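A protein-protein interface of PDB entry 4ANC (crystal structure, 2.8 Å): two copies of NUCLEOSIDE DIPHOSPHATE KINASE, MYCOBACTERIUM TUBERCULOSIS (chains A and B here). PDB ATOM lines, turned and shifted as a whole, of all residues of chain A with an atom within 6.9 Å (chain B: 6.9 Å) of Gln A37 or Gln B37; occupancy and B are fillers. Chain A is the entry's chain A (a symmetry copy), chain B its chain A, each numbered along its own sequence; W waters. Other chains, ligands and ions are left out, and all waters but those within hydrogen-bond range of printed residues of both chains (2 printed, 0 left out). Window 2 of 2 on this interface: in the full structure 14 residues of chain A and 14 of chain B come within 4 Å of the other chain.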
ATOM      1  N   ALA A  35     -28.740 -24.447  24.389  1.00  0.00           N
ATOM      2  CA  ALA A  35     -27.415 -24.960  24.068  1.00  0.00           C
ATOM      3  C   ALA A  35     -26.406 -24.346  25.028  1.00  0.00           C
ATOM      4  O   ALA A  35     -26.629 -23.257  25.555  1.00  0.00           O
ATOM      5  CB  ALA A  35     -27.054 -24.637  22.632  1.00  0.00           C
ATOM      6  N   LEU A  36     -25.299 -25.043  25.255  1.00  0.00           N
ATOM      7  CA  LEU A  36     -24.298 -24.583  26.207  1.00  0.00           C
ATOM      8  C   LEU A  36     -22.981 -25.319  26.002  1.00  0.00           C
ATOM      9  O   LEU A  36     -22.957 -26.549  25.936  1.00  0.00           O
ATOM     10  CB  LEU A  36     -24.796 -24.807  27.634  1.00  0.00           C
ATOM     11  CG  LEU A  36     -23.846 -24.401  28.761  1.00  0.00           C
ATOM     12  CD1 LEU A  36     -23.756 -22.887  28.857  1.00  0.00           C
ATOM     13  CD2 LEU A  36     -24.297 -25.002  30.083  1.00  0.00           C
ATOM     14  N   GLN A  37     -21.886 -24.572  25.908  1.00  0.00           N
ATOM     15  CA  GLN A  37     -20.589 -25.189  25.668  1.00  0.00           C
ATOM     16  C   GLN A  37     -19.415 -24.276  25.999  1.00  0.00           C
ATOM     17  O   GLN A  37     -19.330 -23.154  25.501  1.00  0.00           O
ATOM     18  CB  GLN A  37     -20.486 -25.646  24.208  1.00  0.00           C
ATOM     19  CG  GLN A  37     -19.280 -26.525  23.917  1.00  0.00           C
ATOM     20  CD  GLN A  37     -19.081 -26.769  22.437  1.00  0.00           C
ATOM     21  OE1 GLN A  37     -19.284 -25.876  21.615  1.00  0.00           O
ATOM     22  NE2 GLN A  37     -18.685 -27.986  22.088  1.00  0.00           N
ATOM     23  N   LEU A  38     -18.512 -24.765  26.843  1.00  0.00           N
ATOM     24  CA  LEU A  38     -17.224 -24.115  27.034  1.00  0.00           C
ATOM     25  C   LEU A  38     -16.371 -24.455  25.821  1.00  0.00           C
ATOM     26  O   LEU A  38     -16.205 -25.630  25.485  1.00  0.00           O
ATOM     27  CB  LEU A  38     -16.540 -24.619  28.303  1.00  0.00           C
ATOM     28  CG  LEU A  38     -15.184 -23.992  28.638  1.00  0.00           C
ATOM     29  CD1 LEU A  38     -15.368 -22.726  29.457  1.00  0.00           C
ATOM     30  CD2 LEU A  38     -14.309 -24.981  29.386  1.00  0.00           C
ATOM     31  N   ARG A  39     -15.847 -23.432  25.157  1.00  0.00           N
ATOM     32  CA  ARG A  39     -15.113 -23.638  23.917  1.00  0.00           C
ATOM     33  C   ARG A  39     -14.046 -22.570  23.736  1.00  0.00           C
ATOM     34  O   ARG A  39     -14.083 -21.527  24.387  1.00  0.00           O
ATOM     35  CB  ARG A  39     -16.071 -23.583  22.727  1.00  0.00           C
ATOM     36  CG  ARG A  39     -16.321 -22.170  22.223  1.00  0.00           C
ATOM     37  CD  ARG A  39     -17.576 -22.078  21.372  1.00  0.00           C
ATOM     38  NE  ARG A  39     -17.506 -22.911  20.176  1.00  0.00           N
ATOM     39  CZ  ARG A  39     -16.830 -22.586  19.080  1.00  0.00           C
ATOM     40  NH1 ARG A  39     -16.151 -21.451  19.032  1.00  0.00           N
ATOM     41  NH2 ARG A  39     -16.825 -23.403  18.036  1.00  0.00           N
ATOM     42  N   THR A  40     -13.098 -22.834  22.844  1.00  0.00           N
ATOM     43  CA  THR A  40     -12.097 -21.839  22.489  1.00  0.00           C
ATOM     44  C   THR A  40     -12.539 -21.090  21.235  1.00  0.00           C
ATOM     45  O   THR A  40     -13.395 -21.563  20.487  1.00  0.00           O
ATOM     46  CB  THR A  40     -10.715 -22.476  22.264  1.00  0.00           C
ATOM     47  OG1 THR A  40     -10.841 -23.595  21.379  1.00  0.00           O
ATOM     48  CG2 THR A  40     -10.139 -22.957  23.585  1.00  0.00           C
ATOM     49  N   VAL A  71     -14.254 -19.544  26.448  1.00  0.00           N
ATOM     50  CA  VAL A  71     -15.485 -18.846  26.786  1.00  0.00           C
ATOM     51  C   VAL A  71     -16.633 -19.838  26.879  1.00  0.00           C
ATOM     52  O   VAL A  71     -16.529 -20.971  26.410  1.00  0.00           O
ATOM     53  CB  VAL A  71     -15.846 -17.778  25.738  1.00  0.00           C
ATOM     54  CG1 VAL A  71     -14.689 -16.814  25.552  1.00  0.00           C
ATOM     55  CG2 VAL A  71     -16.213 -18.435  24.422  1.00  0.00           C
ATOM     56  N   VAL A  72     -17.726 -19.409  27.494  1.00  0.00           N
ATOM     57  CA  VAL A  72     -18.923 -20.231  27.572  1.00  0.00           C
ATOM     58  C   VAL A  72     -20.004 -19.652  26.666  1.00  0.00           C
ATOM     59  O   VAL A  72     -20.543 -18.579  26.933  1.00  0.00           O
ATOM     60  CB  VAL A  72     -19.451 -20.328  29.015  1.00  0.00           C
ATOM     61  CG1 VAL A  72     -20.791 -21.042  29.041  1.00  0.00           C
ATOM     62  CG2 VAL A  72     -18.443 -21.039  29.905  1.00  0.00           C
ATOM     63  N   ALA A  73     -20.301 -20.355  25.579  1.00  0.00           N
ATOM     64  CA  ALA A  73     -21.342 -19.930  24.648  1.00  0.00           C
ATOM     65  C   ALA A  73     -22.642 -20.661  24.953  1.00  0.00           C
ATOM     66  O   ALA A  73     -22.625 -21.772  25.471  1.00  0.00           O
ATOM     67  CB  ALA A  73     -20.912 -20.190  23.213  1.00  0.00           C
ATOM     68  N   ALA A  74     -23.767 -20.036  24.625  1.00  0.00           N
ATOM     69  CA  ALA A  74     -25.072 -20.629  24.902  1.00  0.00           C
ATOM     70  C   ALA A  74     -26.191 -20.030  24.058  1.00  0.00           C
ATOM     71  O   ALA A  74     -26.130 -18.869  23.662  1.00  0.00           O
ATOM     72  CB  ALA A  74     -25.406 -20.500  26.383  1.00  0.00           C
ATOM     73  N   ILE A  75     -27.209 -20.839  23.786  1.00  0.00           N
ATOM     74  CA  ILE A  75     -28.428 -20.353  23.157  1.00  0.00           C
ATOM     75  C   ILE A  75     -29.511 -20.280  24.223  1.00  0.00           C
ATOM     76  O   ILE A  75     -29.883 -21.295  24.806  1.00  0.00           O
ATOM     77  CB  ILE A  75     -28.903 -21.286  22.027  1.00  0.00           C
ATOM     78  CG1 ILE A  75     -27.806 -21.461  20.974  1.00  0.00           C
ATOM     79  CG2 ILE A  75     -30.182 -20.752  21.394  1.00  0.00           C
ATOM     80  CD1 ILE A  75     -28.139 -22.479  19.899  1.00  0.00           C
ATOM     81  N   TRP A 132     -21.980 -19.442  16.053  1.00  0.00           N
ATOM     82  CA  TRP A 132     -21.415 -20.174  17.183  1.00  0.00           C
ATOM     83  C   TRP A 132     -21.936 -21.606  17.267  1.00  0.00           C
ATOM     84  O   TRP A 132     -21.235 -22.510  17.724  1.00  0.00           O
ATOM     85  CB  TRP A 132     -21.714 -19.429  18.486  1.00  0.00           C
ATOM     86  CG  TRP A 132     -21.000 -18.123  18.610  1.00  0.00           C
ATOM     87  CD1 TRP A 132     -21.341 -16.940  18.018  1.00  0.00           C
ATOM     88  CD2 TRP A 132     -19.825 -17.860  19.381  1.00  0.00           C
ATOM     89  NE1 TRP A 132     -20.448 -15.959  18.370  1.00  0.00           N
ATOM     90  CE2 TRP A 132     -19.505 -16.499  19.208  1.00  0.00           C
ATOM     91  CE3 TRP A 132     -19.007 -18.646  20.202  1.00  0.00           C
ATOM     92  CZ2 TRP A 132     -18.407 -15.906  19.822  1.00  0.00           C
ATOM     93  CZ3 TRP A 132     -17.916 -18.054  20.811  1.00  0.00           C
ATOM     94  CH2 TRP A 132     -17.626 -16.698  20.618  1.00  0.00           C
ATOM     95  N   PHE A 133     -23.175 -21.802  16.830  1.00  0.00           N
ATOM     96  CA  PHE A 133     -23.786 -23.124  16.821  1.00  0.00           C
ATOM     97  C   PHE A 133     -24.340 -23.441  15.435  1.00  0.00           C
ATOM     98  O   PHE A 133     -25.554 -23.542  15.255  1.00  0.00           O
ATOM     99  CB  PHE A 133     -24.903 -23.207  17.864  1.00  0.00           C
ATOM    100  CG  PHE A 133     -24.429 -23.039  19.279  1.00  0.00           C
ATOM    101  CD1 PHE A 133     -24.326 -21.780  19.845  1.00  0.00           C
ATOM    102  CD2 PHE A 133     -24.090 -24.143  20.043  1.00  0.00           C
ATOM    103  CE1 PHE A 133     -23.894 -21.625  21.140  1.00  0.00           C
ATOM    104  CE2 PHE A 133     -23.655 -23.993  21.343  1.00  0.00           C
ATOM    105  CZ  PHE A 133     -23.558 -22.730  21.892  1.00  0.00           C
ATOM    106  N   ALA B  35     -14.186 -28.471  31.185  1.00  0.00           N
ATOM    107  CA  ALA B  35     -15.029 -28.721  30.024  1.00  0.00           C
ATOM    108  C   ALA B  35     -16.489 -28.623  30.448  1.00  0.00           C
ATOM    109  O   ALA B  35     -16.815 -28.841  31.614  1.00  0.00           O
ATOM    110  CB  ALA B  35     -14.733 -30.086  29.435  1.00  0.00           C
ATOM    111  N   LEU B  36     -17.363 -28.295  29.505  1.00  0.00           N
ATOM    112  CA  LEU B  36     -18.773 -28.107  29.813  1.00  0.00           C
ATOM    113  C   LEU B  36     -19.611 -28.129  28.542  1.00  0.00           C
ATOM    114  O   LEU B  36     -19.300 -27.430  27.577  1.00  0.00           O
ATOM    115  CB  LEU B  36     -18.974 -26.776  30.537  1.00  0.00           C
ATOM    116  CG  LEU B  36     -20.410 -26.411  30.910  1.00  0.00           C
ATOM    117  CD1 LEU B  36     -20.901 -27.289  32.048  1.00  0.00           C
ATOM    118  CD2 LEU B  36     -20.509 -24.939  31.280  1.00  0.00           C
ATOM    119  N   GLN B  37     -20.674 -28.925  28.541  1.00  0.00           N
ATOM    120  CA  GLN B  37     -21.508 -29.044  27.352  1.00  0.00           C
ATOM    121  C   GLN B  37     -22.881 -29.642  27.634  1.00  0.00           C
ATOM    122  O   GLN B  37     -22.990 -30.724  28.206  1.00  0.00           O
ATOM    123  CB  GLN B  37     -20.791 -29.884  26.289  1.00  0.00           C
ATOM    124  CG  GLN B  37     -21.459 -29.857  24.924  1.00  0.00           C
ATOM    125  CD  GLN B  37     -20.867 -30.867  23.965  1.00  0.00           C
ATOM    126  OE1 GLN B  37     -20.523 -31.984  24.354  1.00  0.00           O
ATOM    127  NE2 GLN B  37     -20.740 -30.480  22.703  1.00  0.00           N
ATOM    128  N   LEU B  38     -23.926 -28.928  27.226  1.00  0.00           N
ATOM    129  CA  LEU B  38     -25.264 -29.498  27.192  1.00  0.00           C
ATOM    130  C   LEU B  38     -25.328 -30.407  25.975  1.00  0.00           C
ATOM    131  O   LEU B  38     -25.023 -29.980  24.859  1.00  0.00           O
ATOM    132  CB  LEU B  38     -26.322 -28.402  27.073  1.00  0.00           C
ATOM    133  CG  LEU B  38     -27.780 -28.866  27.055  1.00  0.00           C
ATOM    134  CD1 LEU B  38     -28.322 -28.983  28.469  1.00  0.00           C
ATOM    135  CD2 LEU B  38     -28.634 -27.911  26.241  1.00  0.00           C
ATOM    136  N   ARG B  39     -25.706 -31.662  26.188  1.00  0.00           N
ATOM    137  CA  ARG B  39     -25.689 -32.646  25.116  1.00  0.00           C
ATOM    138  C   ARG B  39     -26.767 -33.697  25.329  1.00  0.00           C
ATOM    139  O   ARG B  39     -27.298 -33.839  26.429  1.00  0.00           O
ATOM    140  CB  ARG B  39     -24.328 -33.339  25.065  1.00  0.00           C
ATOM    141  CG  ARG B  39     -24.222 -34.524  26.011  1.00  0.00           C
ATOM    142  CD  ARG B  39     -22.779 -34.913  26.285  1.00  0.00           C
ATOM    143  NE  ARG B  39     -22.068 -35.317  25.076  1.00  0.00           N
ATOM    144  CZ  ARG B  39     -22.200 -36.505  24.495  1.00  0.00           C
ATOM    145  NH1 ARG B  39     -23.029 -37.403  25.004  1.00  0.00           N
ATOM    146  NH2 ARG B  39     -21.510 -36.789  23.400  1.00  0.00           N
ATOM    147  N   THR B  40     -27.081 -34.436  24.271  1.00  0.00           N
ATOM    148  CA  THR B  40     -28.002 -35.557  24.380  1.00  0.00           C
ATOM    149  C   THR B  40     -27.217 -36.851  24.576  1.00  0.00           C
ATOM    150  O   THR B  40     -26.023 -36.914  24.283  1.00  0.00           O
ATOM    151  CB  THR B  40     -28.909 -35.672  23.144  1.00  0.00           C
ATOM    152  OG1 THR B  40     -28.111 -35.619  21.956  1.00  0.00           O
ATOM    153  CG2 THR B  40     -29.906 -34.525  23.117  1.00  0.00           C
ATOM    154  N   VAL B  71     -28.614 -33.467  28.947  1.00  0.00           N
ATOM    155  CA  VAL B  71     -27.903 -33.342  30.210  1.00  0.00           C
ATOM    156  C   VAL B  71     -26.734 -32.383  30.052  1.00  0.00           C
ATOM    157  O   VAL B  71     -26.323 -32.065  28.936  1.00  0.00           O
ATOM    158  CB  VAL B  71     -27.361 -34.695  30.701  1.00  0.00           C
ATOM    159  CG1 VAL B  71     -28.486 -35.709  30.791  1.00  0.00           C
ATOM    160  CG2 VAL B  71     -26.267 -35.191  29.777  1.00  0.00           C
ATOM    161  N   VAL B  72     -26.205 -31.918  31.175  1.00  0.00           N
ATOM    162  CA  VAL B  72     -25.029 -31.062  31.161  1.00  0.00           C
ATOM    163  C   VAL B  72     -23.826 -31.835  31.692  1.00  0.00           C
ATOM    164  O   VAL B  72     -23.758 -32.161  32.876  1.00  0.00           O
ATOM    165  CB  VAL B  72     -25.243 -29.791  32.002  1.00  0.00           C
ATOM    166  CG1 VAL B  72     -23.947 -29.006  32.114  1.00  0.00           C
ATOM    167  CG2 VAL B  72     -26.344 -28.932  31.399  1.00  0.00           C
ATOM    168  N   ALA B  73     -22.888 -32.147  30.805  1.00  0.00           N
ATOM    169  CA  ALA B  73     -21.669 -32.853  31.189  1.00  0.00           C
ATOM    170  C   ALA B  73     -20.536 -31.859  31.397  1.00  0.00           C
ATOM    171  O   ALA B  73     -20.525 -30.791  30.792  1.00  0.00           O
ATOM    172  CB  ALA B  73     -21.290 -33.876  30.130  1.00  0.00           C
ATOM    173  N   ALA B  74     -19.581 -32.214  32.249  1.00  0.00           N
ATOM    174  CA  ALA B  74     -18.464 -31.324  32.550  1.00  0.00           C
ATOM    175  C   ALA B  74     -17.263 -32.052  33.141  1.00  0.00           C
ATOM    176  O   ALA B  74     -17.410 -33.077  33.803  1.00  0.00           O
ATOM    177  CB  ALA B  74     -18.915 -30.210  33.486  1.00  0.00           C
ATOM    178  N   ILE B  75     -16.075 -31.512  32.891  1.00  0.00           N
ATOM    179  CA  ILE B  75     -14.864 -31.985  33.545  1.00  0.00           C
ATOM    180  C   ILE B  75     -14.471 -30.966  34.604  1.00  0.00           C
ATOM    181  O   ILE B  75     -14.185 -29.814  34.286  1.00  0.00           O
ATOM    182  CB  ILE B  75     -13.699 -32.145  32.550  1.00  0.00           C
ATOM    183  CG1 ILE B  75     -14.086 -33.096  31.415  1.00  0.00           C
ATOM    184  CG2 ILE B  75     -12.447 -32.637  33.267  1.00  0.00           C
ATOM    185  CD1 ILE B  75     -13.047 -33.197  30.314  1.00  0.00           C
ATOM    186  N   TRP B 132     -17.175 -39.451  27.906  1.00  0.00           N
ATOM    187  CA  TRP B 132     -18.009 -38.291  27.609  1.00  0.00           C
ATOM    188  C   TRP B 132     -17.259 -37.222  26.818  1.00  0.00           C
ATOM    189  O   TRP B 132     -17.849 -36.495  26.018  1.00  0.00           O
ATOM    190  CB  TRP B 132     -18.555 -37.697  28.908  1.00  0.00           C
ATOM    191  CG  TRP B 132     -19.537 -38.580  29.608  1.00  0.00           C
ATOM    192  CD1 TRP B 132     -19.256 -39.667  30.385  1.00  0.00           C
ATOM    193  CD2 TRP B 132     -20.961 -38.449  29.603  1.00  0.00           C
ATOM    194  NE1 TRP B 132     -20.418 -40.222  30.861  1.00  0.00           N
ATOM    195  CE2 TRP B 132     -21.481 -39.492  30.393  1.00  0.00           C
ATOM    196  CE3 TRP B 132     -21.850 -37.550  29.003  1.00  0.00           C
ATOM    197  CZ2 TRP B 132     -22.847 -39.663  30.600  1.00  0.00           C
ATOM    198  CZ3 TRP B 132     -23.207 -37.721  29.210  1.00  0.00           C
ATOM    199  CH2 TRP B 132     -23.691 -38.769  30.002  1.00  0.00           C
ATOM    200  N   PHE B 133     -15.956 -37.128  27.057  1.00  0.00           N
ATOM    201  CA  PHE B 133     -15.112 -36.175  26.351  1.00  0.00           C
ATOM    202  C   PHE B 133     -13.910 -36.886  25.738  1.00  0.00           C
ATOM    203  O   PHE B 133     -12.772 -36.663  26.154  1.00  0.00           O
ATOM    204  CB  PHE B 133     -14.642 -35.068  27.297  1.00  0.00           C
ATOM    205  CG  PHE B 133     -15.754 -34.224  27.850  1.00  0.00           C
ATOM    206  CD1 PHE B 133     -16.417 -34.597  29.006  1.00  0.00           C
ATOM    207  CD2 PHE B 133     -16.135 -33.056  27.211  1.00  0.00           C
ATOM    208  CE1 PHE B 133     -17.434 -33.825  29.513  1.00  0.00           C
ATOM    209  CE2 PHE B 133     -17.155 -32.278  27.715  1.00  0.00           C
ATOM    210  CZ  PHE B 133     -17.806 -32.664  28.870  1.00  0.00           C
HETATM  211  O   HOH W   1     -16.041 -27.923  26.907  1.00  0.00           O
HETATM  212  O   HOH W   2     -25.276 -27.544  23.713  1.00  0.00           O
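The side-chain amide nitrogen (NE2) of Gln A37 sits close to the side-chain amide nitrogen (NE2) of Gln B37 (3.3 Å). The backbone NH of Leu B38 lies within hydrogen-bond range of the backbone carbonyl oxygen of Leu A36 (2.9 Å). O of Leu B36 lies within hydrogen-bond range of N of Leu A38 (2.9 Å).
The backbone carbonyl oxygen (O) of Ala B73 sits at hydrogen-bond distance from the backbone NH (N) of Gln B37 (2.9 Å). The backbone NH (N) of Gln A37 lies within hydrogen-bond range of the backbone carbonyl oxygen (O) of Ala A73 (2.9 Å). O of Ala B35 is in hydrogen-bond range of N of Ile B75 (3.1 Å). The backbone carbonyl oxygen (O) of Ala A35 is in hydrogen-bond range of the backbone NH (N) of Ile A75 (3.1 Å).
Ala A35 touches Leu B38. Leu B36 touches Leu A36 (CD2 to CD2, 3.97 Å). CA of Gln B37 touches O of Leu A36 (3.2 Å). Leu B36 touches Gln A37. Leu A38 touches Ala B35 (CD2 to CA, 3.9 Å).
Gln A37 touches just these residues of chain B: Leu B36 (3.2 Å) and Gln B37 (3.3 Å). Gln B37 touches two residues of chain A. Printed residues of chain B within 4 Å of Leu A38: Ala B35 (3.9 Å) and Leu B36 (2.9 Å). Printed residues of chain B within 4 Å of Ala A35: Leu B38.
Of the 13 printed residues of chain B, 4 touch a printed residue of chain A. Along chain B the printed residues that touch a printed residue of chain A span positions 35 to 38. Hydrophobic or aromatic side chains of chain A within 4 Å of the printed part of chain B: Leu A36 and Leu A38. Among the printed residues, 8 pairs touch across the chains.
Ala A35 touches Leu B38, and with the chains exchanged Leu A38 touches Ala B35. Leu A36 touches its own counterpart, Leu B36. Leu A36 touches Gln B37, and with the chains exchanged Gln A37 touches Leu B36. Gln A37 touches its own counterpart, Gln B37. Positions printed for both chains: 35, 36, 37, 38, 39, 40, 71, 72, 73, 74, 75, 132 and 133. Of the 8 pairs that touch across the chains among the printed residues, 8 have their exchanged pair printed and touching as well.
Water W1 lies within hydrogen-bond range of the backbone carbonyl oxygen of Leu A38 (2.7 Å) and the backbone NH of Leu B36 (2.9 Å). Water W2 lies within hydrogen-bond range of the backbone carbonyl oxygen (O) of Leu B38 (2.7 Å) and the backbone NH (N) of Leu A36 (2.9 Å).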
